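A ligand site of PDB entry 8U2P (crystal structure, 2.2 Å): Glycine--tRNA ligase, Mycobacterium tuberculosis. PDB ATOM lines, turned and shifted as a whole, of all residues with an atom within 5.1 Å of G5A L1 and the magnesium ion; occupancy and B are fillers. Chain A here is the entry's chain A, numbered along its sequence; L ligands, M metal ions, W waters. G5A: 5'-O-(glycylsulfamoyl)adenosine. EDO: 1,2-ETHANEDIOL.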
ATOM      1  N   PRO A 177     -15.990  19.764  20.041  1.00  0.00           N
ATOM      2  CA  PRO A 177     -15.233  19.923  18.791  1.00  0.00           C
ATOM      3  C   PRO A 177     -15.513  18.827  17.779  1.00  0.00           C
ATOM      4  O   PRO A 177     -15.090  18.955  16.614  1.00  0.00           O
ATOM      5  CB  PRO A 177     -13.769  19.872  19.269  1.00  0.00           C
ATOM      6  CG  PRO A 177     -13.815  18.968  20.472  1.00  0.00           C
ATOM      7  CD  PRO A 177     -15.137  19.293  21.145  1.00  0.00           C
ATOM      8  N   GLU A 178     -16.200  17.761  18.173  1.00  0.00           N
ATOM      9  CA  GLU A 178     -16.672  16.722  17.267  1.00  0.00           C
ATOM     10  C   GLU A 178     -17.968  16.172  17.842  1.00  0.00           C
ATOM     11  O   GLU A 178     -18.224  16.290  19.044  1.00  0.00           O
ATOM     12  CB  GLU A 178     -15.636  15.608  17.072  1.00  0.00           C
ATOM     13  CG  GLU A 178     -15.270  14.848  18.353  1.00  0.00           C
ATOM     14  CD  GLU A 178     -14.381  13.626  18.115  1.00  0.00           C
ATOM     15  OE1 GLU A 178     -13.993  13.366  16.949  1.00  0.00           O
ATOM     16  OE2 GLU A 178     -14.072  12.923  19.098  1.00  0.00           O
ATOM     17  N   ALA A 180     -18.661  12.951  17.657  1.00  0.00           N
ATOM     18  CA  ALA A 180     -18.464  11.527  17.907  1.00  0.00           C
ATOM     19  C   ALA A 180     -18.683  11.159  19.365  1.00  0.00           C
ATOM     20  O   ALA A 180     -19.259  10.104  19.671  1.00  0.00           O
ATOM     21  CB  ALA A 180     -17.060  11.114  17.456  1.00  0.00           C
ATOM     22  N   ARG A 210     -14.677  24.750  16.868  1.00  0.00           N
ATOM     23  CA  ARG A 210     -13.230  24.712  17.053  1.00  0.00           C
ATOM     24  C   ARG A 210     -12.662  26.109  16.907  1.00  0.00           C
ATOM     25  O   ARG A 210     -13.033  26.847  15.988  1.00  0.00           O
ATOM     26  CB  ARG A 210     -12.565  23.754  16.063  1.00  0.00           C
ATOM     27  CG  ARG A 210     -13.052  22.341  16.182  1.00  0.00           C
ATOM     28  CD  ARG A 210     -12.388  21.433  15.171  1.00  0.00           C
ATOM     29  NE  ARG A 210     -12.987  20.100  15.206  1.00  0.00           N
ATOM     30  CZ  ARG A 210     -12.566  19.072  14.496  1.00  0.00           C
ATOM     31  NH1 ARG A 210     -11.529  19.165  13.697  1.00  0.00           N
ATOM     32  NH2 ARG A 210     -13.215  17.914  14.596  1.00  0.00           N
ATOM     33  N   GLU A 212     -10.368  27.699  15.545  1.00  0.00           N
ATOM     34  CA  GLU A 212      -9.379  27.717  14.471  1.00  0.00           C
ATOM     35  C   GLU A 212      -8.559  28.999  14.538  1.00  0.00           C
ATOM     36  O   GLU A 212      -9.104  30.091  14.722  1.00  0.00           O
ATOM     37  CB  GLU A 212     -10.085  27.603  13.116  1.00  0.00           C
ATOM     38  CG  GLU A 212     -10.935  26.333  12.946  1.00  0.00           C
ATOM     39  CD  GLU A 212     -10.123  25.078  12.727  1.00  0.00           C
ATOM     40  OE1 GLU A 212      -8.911  25.194  12.445  1.00  0.00           O
ATOM     41  OE2 GLU A 212     -10.682  23.973  12.837  1.00  0.00           O
ATOM     42  N   ILE A 219     -16.259  28.987   3.481  1.00  0.00           N
ATOM     43  CA  ILE A 219     -16.858  28.142   4.502  1.00  0.00           C
ATOM     44  C   ILE A 219     -16.066  26.857   4.709  1.00  0.00           C
ATOM     45  O   ILE A 219     -16.517  25.950   5.426  1.00  0.00           O
ATOM     46  CB  ILE A 219     -18.331  27.831   4.196  1.00  0.00           C
ATOM     47  CG1 ILE A 219     -18.468  26.934   2.956  1.00  0.00           C
ATOM     48  CG2 ILE A 219     -19.107  29.115   3.977  1.00  0.00           C
ATOM     49  CD1 ILE A 219     -19.907  26.611   2.596  1.00  0.00           C
ATOM     50  N   PHE A 220     -14.868  26.754   4.113  1.00  0.00           N
ATOM     51  CA  PHE A 220     -14.076  25.539   4.248  1.00  0.00           C
ATOM     52  C   PHE A 220     -13.584  25.350   5.675  1.00  0.00           C
ATOM     53  O   PHE A 220     -13.604  24.225   6.198  1.00  0.00           O
ATOM     54  CB  PHE A 220     -12.896  25.570   3.265  1.00  0.00           C
ATOM     55  CG  PHE A 220     -11.937  24.421   3.425  1.00  0.00           C
ATOM     56  CD1 PHE A 220     -12.182  23.190   2.836  1.00  0.00           C
ATOM     57  CD2 PHE A 220     -10.767  24.576   4.155  1.00  0.00           C
ATOM     58  CE1 PHE A 220     -11.284  22.126   2.975  1.00  0.00           C
ATOM     59  CE2 PHE A 220      -9.862  23.522   4.301  1.00  0.00           C
ATOM     60  CZ  PHE A 220     -10.134  22.304   3.709  1.00  0.00           C
ATOM     61  N   ARG A 221     -13.152  26.424   6.320  1.00  0.00           N
ATOM     62  CA  ARG A 221     -12.598  26.360   7.681  1.00  0.00           C
ATOM     63  C   ARG A 221     -13.222  27.485   8.497  1.00  0.00           C
ATOM     64  O   ARG A 221     -12.833  28.656   8.361  1.00  0.00           O
ATOM     65  CB  ARG A 221     -11.072  26.466   7.660  1.00  0.00           C
ATOM     66  CG  ARG A 221     -10.416  26.363   9.026  1.00  0.00           C
ATOM     67  CD  ARG A 221      -8.896  26.571   8.940  1.00  0.00           C
ATOM     68  NE  ARG A 221      -8.364  26.208   7.626  1.00  0.00           N
ATOM     69  CZ  ARG A 221      -8.118  27.064   6.645  1.00  0.00           C
ATOM     70  NH1 ARG A 221      -8.269  28.372   6.799  1.00  0.00           N
ATOM     71  NH2 ARG A 221      -7.717  26.602   5.468  1.00  0.00           N
ATOM     72  N   THR A 222     -14.188  27.135   9.348  1.00  0.00           N
ATOM     73  CA  THR A 222     -14.880  28.096  10.192  1.00  0.00           C
ATOM     74  C   THR A 222     -14.837  27.605  11.636  1.00  0.00           C
ATOM     75  O   THR A 222     -14.540  26.444  11.902  1.00  0.00           O
ATOM     76  CB  THR A 222     -16.333  28.286   9.729  1.00  0.00           C
ATOM     77  OG1 THR A 222     -17.043  27.053   9.872  1.00  0.00           O
ATOM     78  CG2 THR A 222     -16.368  28.697   8.272  1.00  0.00           C
ATOM     79  N   PHE A 225     -19.270  24.990  12.532  1.00  0.00           N
ATOM     80  CA  PHE A 225     -19.550  24.226  11.325  1.00  0.00           C
ATOM     81  C   PHE A 225     -20.376  23.013  11.705  1.00  0.00           C
ATOM     82  O   PHE A 225     -20.566  22.714  12.888  1.00  0.00           O
ATOM     83  CB  PHE A 225     -18.252  23.824  10.614  1.00  0.00           C
ATOM     84  CG  PHE A 225     -17.338  22.997  11.464  1.00  0.00           C
ATOM     85  CD1 PHE A 225     -16.541  23.596  12.435  1.00  0.00           C
ATOM     86  CD2 PHE A 225     -17.264  21.626  11.301  1.00  0.00           C
ATOM     87  CE1 PHE A 225     -15.701  22.836  13.220  1.00  0.00           C
ATOM     88  CE2 PHE A 225     -16.424  20.857  12.086  1.00  0.00           C
ATOM     89  CZ  PHE A 225     -15.640  21.466  13.056  1.00  0.00           C
ATOM     90  N   GLN A 227     -21.154  18.807  11.040  1.00  0.00           N
ATOM     91  CA  GLN A 227     -20.560  17.542  10.649  1.00  0.00           C
ATOM     92  C   GLN A 227     -21.645  16.493  10.453  1.00  0.00           C
ATOM     93  O   GLN A 227     -22.739  16.588  11.003  1.00  0.00           O
ATOM     94  CB  GLN A 227     -19.568  17.029  11.690  1.00  0.00           C
ATOM     95  CG  GLN A 227     -18.406  17.949  11.995  1.00  0.00           C
ATOM     96  CD  GLN A 227     -17.440  17.329  12.985  1.00  0.00           C
ATOM     97  OE1 GLN A 227     -17.811  17.025  14.120  1.00  0.00           O
ATOM     98  NE2 GLN A 227     -16.212  17.122  12.550  1.00  0.00           N
ATOM     99  N   GLU A 229     -21.412  12.566  10.962  1.00  0.00           N
ATOM    100  CA  GLU A 229     -20.516  11.541  11.477  1.00  0.00           C
ATOM    101  C   GLU A 229     -21.305  10.285  11.811  1.00  0.00           C
ATOM    102  O   GLU A 229     -22.444  10.353  12.293  1.00  0.00           O
ATOM    103  CB  GLU A 229     -19.772  12.033  12.728  1.00  0.00           C
ATOM    104  CG  GLU A 229     -19.116  13.402  12.535  1.00  0.00           C
ATOM    105  CD  GLU A 229     -18.132  13.773  13.634  1.00  0.00           C
ATOM    106  OE1 GLU A 229     -18.496  13.700  14.833  1.00  0.00           O
ATOM    107  OE2 GLU A 229     -16.991  14.156  13.300  1.00  0.00           O
ATOM    108  N   HIS A 269      -3.378   9.383   5.868  1.00  0.00           N
ATOM    109  CA  HIS A 269      -2.585  10.143   6.817  1.00  0.00           C
ATOM    110  C   HIS A 269      -1.291   9.396   7.110  1.00  0.00           C
ATOM    111  O   HIS A 269      -1.315   8.182   7.335  1.00  0.00           O
ATOM    112  CB  HIS A 269      -3.352  10.346   8.127  1.00  0.00           C
ATOM    113  CG  HIS A 269      -4.545  11.255   8.022  1.00  0.00           C
ATOM    114  ND1 HIS A 269      -5.078  11.890   9.113  1.00  0.00           N
ATOM    115  CD2 HIS A 269      -5.306  11.607   6.964  1.00  0.00           C
ATOM    116  CE1 HIS A 269      -6.129  12.616   8.726  1.00  0.00           C
ATOM    117  NE2 HIS A 269      -6.288  12.454   7.429  1.00  0.00           N
ATOM    118  N   TYR A 277      -7.033   9.646  18.410  1.00  0.00           N
ATOM    119  CA  TYR A 277      -8.018   8.578  18.530  1.00  0.00           C
ATOM    120  C   TYR A 277      -7.956   7.563  17.390  1.00  0.00           C
ATOM    121  O   TYR A 277      -8.716   6.586  17.413  1.00  0.00           O
ATOM    122  CB  TYR A 277      -9.439   9.164  18.608  1.00  0.00           C
ATOM    123  CG  TYR A 277      -9.710  10.216  17.556  1.00  0.00           C
ATOM    124  CD1 TYR A 277      -9.904   9.867  16.222  1.00  0.00           C
ATOM    125  CD2 TYR A 277      -9.771  11.565  17.898  1.00  0.00           C
ATOM    126  CE1 TYR A 277     -10.149  10.836  15.258  1.00  0.00           C
ATOM    127  CE2 TYR A 277     -10.010  12.534  16.942  1.00  0.00           C
ATOM    128  CZ  TYR A 277     -10.200  12.164  15.629  1.00  0.00           C
ATOM    129  OH  TYR A 277     -10.440  13.143  14.687  1.00  0.00           O
ATOM    130  N   ASP A 283      -8.510  10.183   4.073  1.00  0.00           N
ATOM    131  CA  ASP A 283      -9.316  11.359   3.766  1.00  0.00           C
ATOM    132  C   ASP A 283      -9.816  11.288   2.326  1.00  0.00           C
ATOM    133  O   ASP A 283      -9.060  10.965   1.413  1.00  0.00           O
ATOM    134  CB  ASP A 283      -8.529  12.655   3.951  1.00  0.00           C
ATOM    135  CG  ASP A 283      -8.414  13.071   5.404  1.00  0.00           C
ATOM    136  OD1 ASP A 283      -8.976  12.384   6.279  1.00  0.00           O
ATOM    137  OD2 ASP A 283      -7.750  14.105   5.655  1.00  0.00           O
ATOM    138  N   GLU A 297      -9.368  18.487   2.348  1.00  0.00           N
ATOM    139  CA  GLU A 297     -10.084  17.413   3.010  1.00  0.00           C
ATOM    140  C   GLU A 297     -11.588  17.646   2.910  1.00  0.00           C
ATOM    141  O   GLU A 297     -12.097  18.683   3.319  1.00  0.00           O
ATOM    142  CB  GLU A 297      -9.665  17.330   4.478  1.00  0.00           C
ATOM    143  CG  GLU A 297     -10.363  16.224   5.276  1.00  0.00           C
ATOM    144  CD  GLU A 297     -10.027  16.259   6.756  1.00  0.00           C
ATOM    145  OE1 GLU A 297      -9.125  17.021   7.155  1.00  0.00           O
ATOM    146  OE2 GLU A 297     -10.663  15.509   7.531  1.00  0.00           O
ATOM    147  N   LEU A 298     -12.285  16.665   2.357  1.00  0.00           N
ATOM    148  CA  LEU A 298     -13.744  16.683   2.321  1.00  0.00           C
ATOM    149  C   LEU A 298     -14.366  15.840   3.425  1.00  0.00           C
ATOM    150  O   LEU A 298     -15.393  16.230   3.994  1.00  0.00           O
ATOM    151  CB  LEU A 298     -14.232  16.190   0.955  1.00  0.00           C
ATOM    152  CG  LEU A 298     -15.705  16.391   0.610  1.00  0.00           C
ATOM    153  CD1 LEU A 298     -16.075  17.848   0.733  1.00  0.00           C
ATOM    154  CD2 LEU A 298     -15.978  15.868  -0.789  1.00  0.00           C
ATOM    155  N   GLU A 299     -13.745  14.710   3.754  1.00  0.00           N
ATOM    156  CA  GLU A 299     -14.283  13.790   4.746  1.00  0.00           C
ATOM    157  C   GLU A 299     -13.163  12.877   5.192  1.00  0.00           C
ATOM    158  O   GLU A 299     -12.294  12.522   4.392  1.00  0.00           O
ATOM    159  CB  GLU A 299     -15.457  12.982   4.176  1.00  0.00           C
ATOM    160  CG  GLU A 299     -15.838  11.768   4.996  1.00  0.00           C
ATOM    161  CD  GLU A 299     -17.152  11.142   4.552  1.00  0.00           C
ATOM    162  OE1 GLU A 299     -17.695  11.555   3.502  1.00  0.00           O
ATOM    163  OE2 GLU A 299     -17.644  10.229   5.250  1.00  0.00           O
ATOM    164  N   GLY A 300     -13.176  12.502   6.459  1.00  0.00           N
ATOM    165  CA  GLY A 300     -12.227  11.563   7.015  1.00  0.00           C
ATOM    166  C   GLY A 300     -12.926  10.277   7.416  1.00  0.00           C
ATOM    167  O   GLY A 300     -13.979  10.297   8.056  1.00  0.00           O
ATOM    168  N   ARG A 304     -10.867   4.005  14.529  1.00  0.00           N
ATOM    169  CA  ARG A 304     -10.611   4.449  15.898  1.00  0.00           C
ATOM    170  C   ARG A 304     -10.427   3.285  16.870  1.00  0.00           C
ATOM    171  O   ARG A 304     -10.403   3.509  18.088  1.00  0.00           O
ATOM    172  CB  ARG A 304     -11.731   5.369  16.377  1.00  0.00           C
ATOM    173  CG  ARG A 304     -11.919   6.604  15.489  1.00  0.00           C
ATOM    174  CD  ARG A 304     -13.142   7.412  15.901  1.00  0.00           C
ATOM    175  NE  ARG A 304     -12.923   8.161  17.129  1.00  0.00           N
ATOM    176  CZ  ARG A 304     -13.085   9.480  17.268  1.00  0.00           C
ATOM    177  NH1 ARG A 304     -13.487  10.242  16.260  1.00  0.00           N
ATOM    178  NH2 ARG A 304     -12.851  10.037  18.456  1.00  0.00           N
ATOM    179  N   GLU A 337     -15.186   5.120  11.412  1.00  0.00           N
ATOM    180  CA  GLU A 337     -15.899   6.387  11.513  1.00  0.00           C
ATOM    181  C   GLU A 337     -15.781   7.205  10.233  1.00  0.00           C
ATOM    182  O   GLU A 337     -14.730   7.826  10.002  1.00  0.00           O
ATOM    183  CB  GLU A 337     -15.395   7.222  12.686  1.00  0.00           C
ATOM    184  CG  GLU A 337     -16.128   8.560  12.834  1.00  0.00           C
ATOM    185  CD  GLU A 337     -15.402   9.577  13.689  1.00  0.00           C
ATOM    186  OE1 GLU A 337     -14.160   9.679  13.573  1.00  0.00           O
ATOM    187  OE2 GLU A 337     -16.068  10.275  14.467  1.00  0.00           O
ATOM    188  N   ALA A 339     -16.576  10.633   8.841  1.00  0.00           N
ATOM    189  CA  ALA A 339     -16.869  11.931   9.442  1.00  0.00           C
ATOM    190  C   ALA A 339     -16.771  12.981   8.338  1.00  0.00           C
ATOM    191  O   ALA A 339     -15.673  13.378   7.949  1.00  0.00           O
ATOM    192  CB  ALA A 339     -15.916  12.245  10.589  1.00  0.00           C
ATOM    193  N   ALA A 340     -17.928  13.416   7.834  1.00  0.00           N
ATOM    194  CA  ALA A 340     -17.982  14.359   6.727  1.00  0.00           C
ATOM    195  C   ALA A 340     -18.283  15.769   7.227  1.00  0.00           C
ATOM    196  O   ALA A 340     -18.873  15.967   8.294  1.00  0.00           O
ATOM    197  CB  ALA A 340     -19.058  13.945   5.710  1.00  0.00           C
ATOM    198  N   GLY A 341     -17.860  16.748   6.435  1.00  0.00           N
ATOM    199  CA  GLY A 341     -18.196  18.132   6.704  1.00  0.00           C
ATOM    200  C   GLY A 341     -19.381  18.571   5.877  1.00  0.00           C
ATOM    201  O   GLY A 341     -19.300  18.629   4.648  1.00  0.00           O
ATOM    202  N   THR A 343     -20.774  21.575   5.703  1.00  0.00           N
ATOM    203  CA  THR A 343     -20.547  22.863   5.052  1.00  0.00           C
ATOM    204  C   THR A 343     -19.462  22.781   3.996  1.00  0.00           C
ATOM    205  O   THR A 343     -19.481  23.560   3.029  1.00  0.00           O
ATOM    206  CB  THR A 343     -20.205  23.923   6.114  1.00  0.00           C
ATOM    207  OG1 THR A 343     -19.111  23.452   6.910  1.00  0.00           O
ATOM    208  CG2 THR A 343     -21.402  24.165   7.015  1.00  0.00           C
ATOM    209  N   ARG A 344     -18.497  21.863   4.155  1.00  0.00           N
ATOM    210  CA  ARG A 344     -17.487  21.668   3.112  1.00  0.00           C
ATOM    211  C   ARG A 344     -18.071  20.941   1.909  1.00  0.00           C
ATOM    212  O   ARG A 344     -17.720  21.245   0.764  1.00  0.00           O
ATOM    213  CB  ARG A 344     -16.295  20.888   3.665  1.00  0.00           C
ATOM    214  CG  ARG A 344     -15.225  21.745   4.309  1.00  0.00           C
ATOM    215  CD  ARG A 344     -13.962  20.940   4.585  1.00  0.00           C
ATOM    216  NE  ARG A 344     -13.107  21.614   5.541  1.00  0.00           N
ATOM    217  CZ  ARG A 344     -12.038  21.076   6.107  1.00  0.00           C
ATOM    218  NH1 ARG A 344     -11.609  19.865   5.776  1.00  0.00           N
ATOM    219  NH2 ARG A 344     -11.379  21.758   7.042  1.00  0.00           N
HETATM  220  C   G5A L   1     -13.516  14.253  13.077  1.00  0.00           C
HETATM  221  N   G5A L   1     -14.974  12.910  14.364  1.00  0.00           N
HETATM  222  O   G5A L   1     -13.926  15.260  13.596  1.00  0.00           O
HETATM  223  S   G5A L   1     -12.083  15.729  11.395  1.00  0.00           S
HETATM  224  N1  G5A L   1     -14.649  23.994   9.394  1.00  0.00           N
HETATM  225  C2  G5A L   1     -15.407  23.280   8.562  1.00  0.00           C
HETATM  226  N3  G5A L   1     -15.443  21.969   8.416  1.00  0.00           N
HETATM  227  C4  G5A L   1     -14.600  21.360   9.236  1.00  0.00           C
HETATM  228  C5  G5A L   1     -13.754  21.964  10.156  1.00  0.00           C
HETATM  229  C6  G5A L   1     -13.808  23.364  10.213  1.00  0.00           C
HETATM  230  N6  G5A L   1     -13.049  24.087  11.045  1.00  0.00           N
HETATM  231  N7  G5A L   1     -13.018  21.024  10.831  1.00  0.00           N
HETATM  232  C8  G5A L   1     -13.407  19.895  10.340  1.00  0.00           C
HETATM  233  N9  G5A L   1     -14.362  20.013   9.369  1.00  0.00           N
HETATM  234  CA  G5A L   1     -13.876  12.857  13.479  1.00  0.00           C
HETATM  235  C1' G5A L   1     -15.015  18.979   8.621  1.00  0.00           C
HETATM  236  O1S G5A L   1     -11.251  15.319  10.299  1.00  0.00           O
HETATM  237  C2' G5A L   1     -14.223  18.422   7.444  1.00  0.00           C
HETATM  238  O2' G5A L   1     -15.076  18.200   6.365  1.00  0.00           O
HETATM  239  O2S G5A L   1     -11.590  16.555  12.461  1.00  0.00           O
HETATM  240  C3' G5A L   1     -13.607  17.151   8.037  1.00  0.00           C
HETATM  241  O3' G5A L   1     -13.385  16.182   7.042  1.00  0.00           O
HETATM  242  N3S G5A L   1     -12.641  14.300  12.018  1.00  0.00           N
HETATM  243  C4' G5A L   1     -14.752  16.686   8.933  1.00  0.00           C
HETATM  244  O4' G5A L   1     -15.291  17.886   9.480  1.00  0.00           O
HETATM  245  C5' G5A L   1     -14.289  15.748  10.019  1.00  0.00           C
HETATM  246  O5' G5A L   1     -13.384  16.458  10.888  1.00  0.00           O
HETATM  247  C1  EDO L   2      -6.188  16.761   7.771  1.00  0.00           C
HETATM  248  O1  EDO L   2      -6.833  15.512   7.837  1.00  0.00           O
HETATM  249  C2  EDO L   2      -6.606  17.596   8.952  1.00  0.00           C
HETATM  250  O2  EDO L   2      -6.421  16.852  10.135  1.00  0.00           O
HETATM  251 MG    MG M   1      -9.227  15.818   9.227  1.00  0.00          MG
HETATM  252  O   HOH W   1     -10.024  17.662   9.913  1.00  0.00           O
HETATM  253  O   HOH W   2      -8.603  15.023  11.056  1.00  0.00           O
HETATM  254  O   HOH W   3     -10.254  21.669  12.206  1.00  0.00           O
HETATM  255  O   HOH W   4      -9.458  13.350   8.882  1.00  0.00           O
HETATM  256  O   HOH W   5     -10.211  15.661  15.089  1.00  0.00           O
HETATM  257  O   HOH W   6     -17.803  21.167   7.206  1.00  0.00           O
HETATM  258  O   HOH W   7     -11.449  12.153  10.530  1.00  0.00           O
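A nitrogen (N6) of G5A L1 is in hydrogen-bond range of the backbone carbonyl oxygen (O) of Thr 222.
The side-chain amide nitrogen of Gln 227 sits at hydrogen-bond distance from an oxygen (O) of G5A L1 (3.1 Å).
N of G5A L1 lies within salt-bridge range of OE1 of Glu 178 (2.8 Å).
The side-chain carboxylate (OE2) of Glu 229 is in salt-bridge range of a nitrogen (N) of G5A L1 (2.6 Å).
NH1 of Arg 210 is in hydrogen-bond range of O2S of G5A L1, 2.9 Å away.
The backbone NH of Thr 222 sits at hydrogen-bond distance from a nitrogen (N1) of G5A L1, 3.2 Å away.
N of G5A L1 is in salt-bridge range of OE2 of Glu 337.
The backbone carbonyl oxygen of Leu 298 is in hydrogen-bond range of an oxygen (O2') of G5A L1, at 3.1 Å.
The side-chain carboxylate (OE2) of Glu 212 is in hydrogen-bond range of a nitrogen (N6) of G5A L1 (3.0 Å).
N of Gly 341 lies close to O2' of G5A L1.
The side-chain carboxylate of Glu 229 lies within hydrogen-bond range of the backbone NH of Ala 180 (2.9 Å).
The guanidinium group (NH1) of Arg 304 lies within salt-bridge range of the side-chain carboxylate (OE1) of Glu 337.
The backbone carbonyl oxygen (O) of Phe 220 sits at hydrogen-bond distance from the guanidinium group (NE) of Arg 344 (2.7 Å).
O of Glu 297 sits at hydrogen-bond distance from NH1 of Arg 344 (2.8 Å).
The backbone NH (N) of Ala 339 sits at hydrogen-bond distance from the backbone carbonyl oxygen (O) of Gly 300 (2.7 Å).
O of Pro 177 is in hydrogen-bond range of NE of Arg 210 (2.8 Å).
OE2 of Glu 178 is in salt-bridge range of NH2 of Arg 304, 3.2 Å away.
OE2 of Glu 229 lies close to OE1 of Gln 227, at 3.1 Å.
The backbone carbonyl oxygen (O) of Phe 220 sits close to a nitrogen (N1) of G5A L1 (3.4 Å).
CA of Arg 221 touches N1 of G5A L1 (3.6 Å).
Phe 225 touches G5A L1 (CD2 to C4, 3.4 Å).
OH of Tyr 277 touches C of G5A L1, 3.6 Å away.
Glu 299 touches G5A L1 (CA to O3', 3.4 Å).
N of Gly 300 touches O3' of G5A L1, at 3.7 Å.
Arg 304 touches G5A L1 (NH1 to N, 3.6 Å).
Ala 339 touches G5A L1.
Arg 344 touches G5A L1.
Hydrophobic or aromatic side chains that line G5A L1: Phe 225 and Ala 339.
One residue has an atom within 4 Å of the magnesium ion: Glu 297.
The magnesium ion is bound by water W2 (2.1 Å), water W1 (2.1 Å), the side-chain carboxylate (OE2) of Glu 297 (2.2 Å), an oxygen (O1S) of G5A L1 (2.3 Å), the side-chain carboxylate (OE1) of Glu 297 (2.4 Å) and water W4 (2.5 Å).
The magnesium ion has six donor atoms within binding distance.
Slightly farther from the magnesium ion lies O1 of EDO L2 (2.8 Å).
Water W6 lies within hydrogen-bond range of the side-chain hydroxyl of Thr 343, a nitrogen (N3) of G5A L1 and the backbone NH of Arg 344.
Water W5 bridges OH of Tyr 277 (2.6 Å) and O2S of G5A L1 (3.1 Å).
Water W3 lies within hydrogen-bond range of the side-chain carboxylate (OE2) of Glu 212 (2.4 Å), a nitrogen (N7) of G5A L1 (3.2 Å) and the guanidinium group (NH1) of Arg 210 (3.2 Å).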
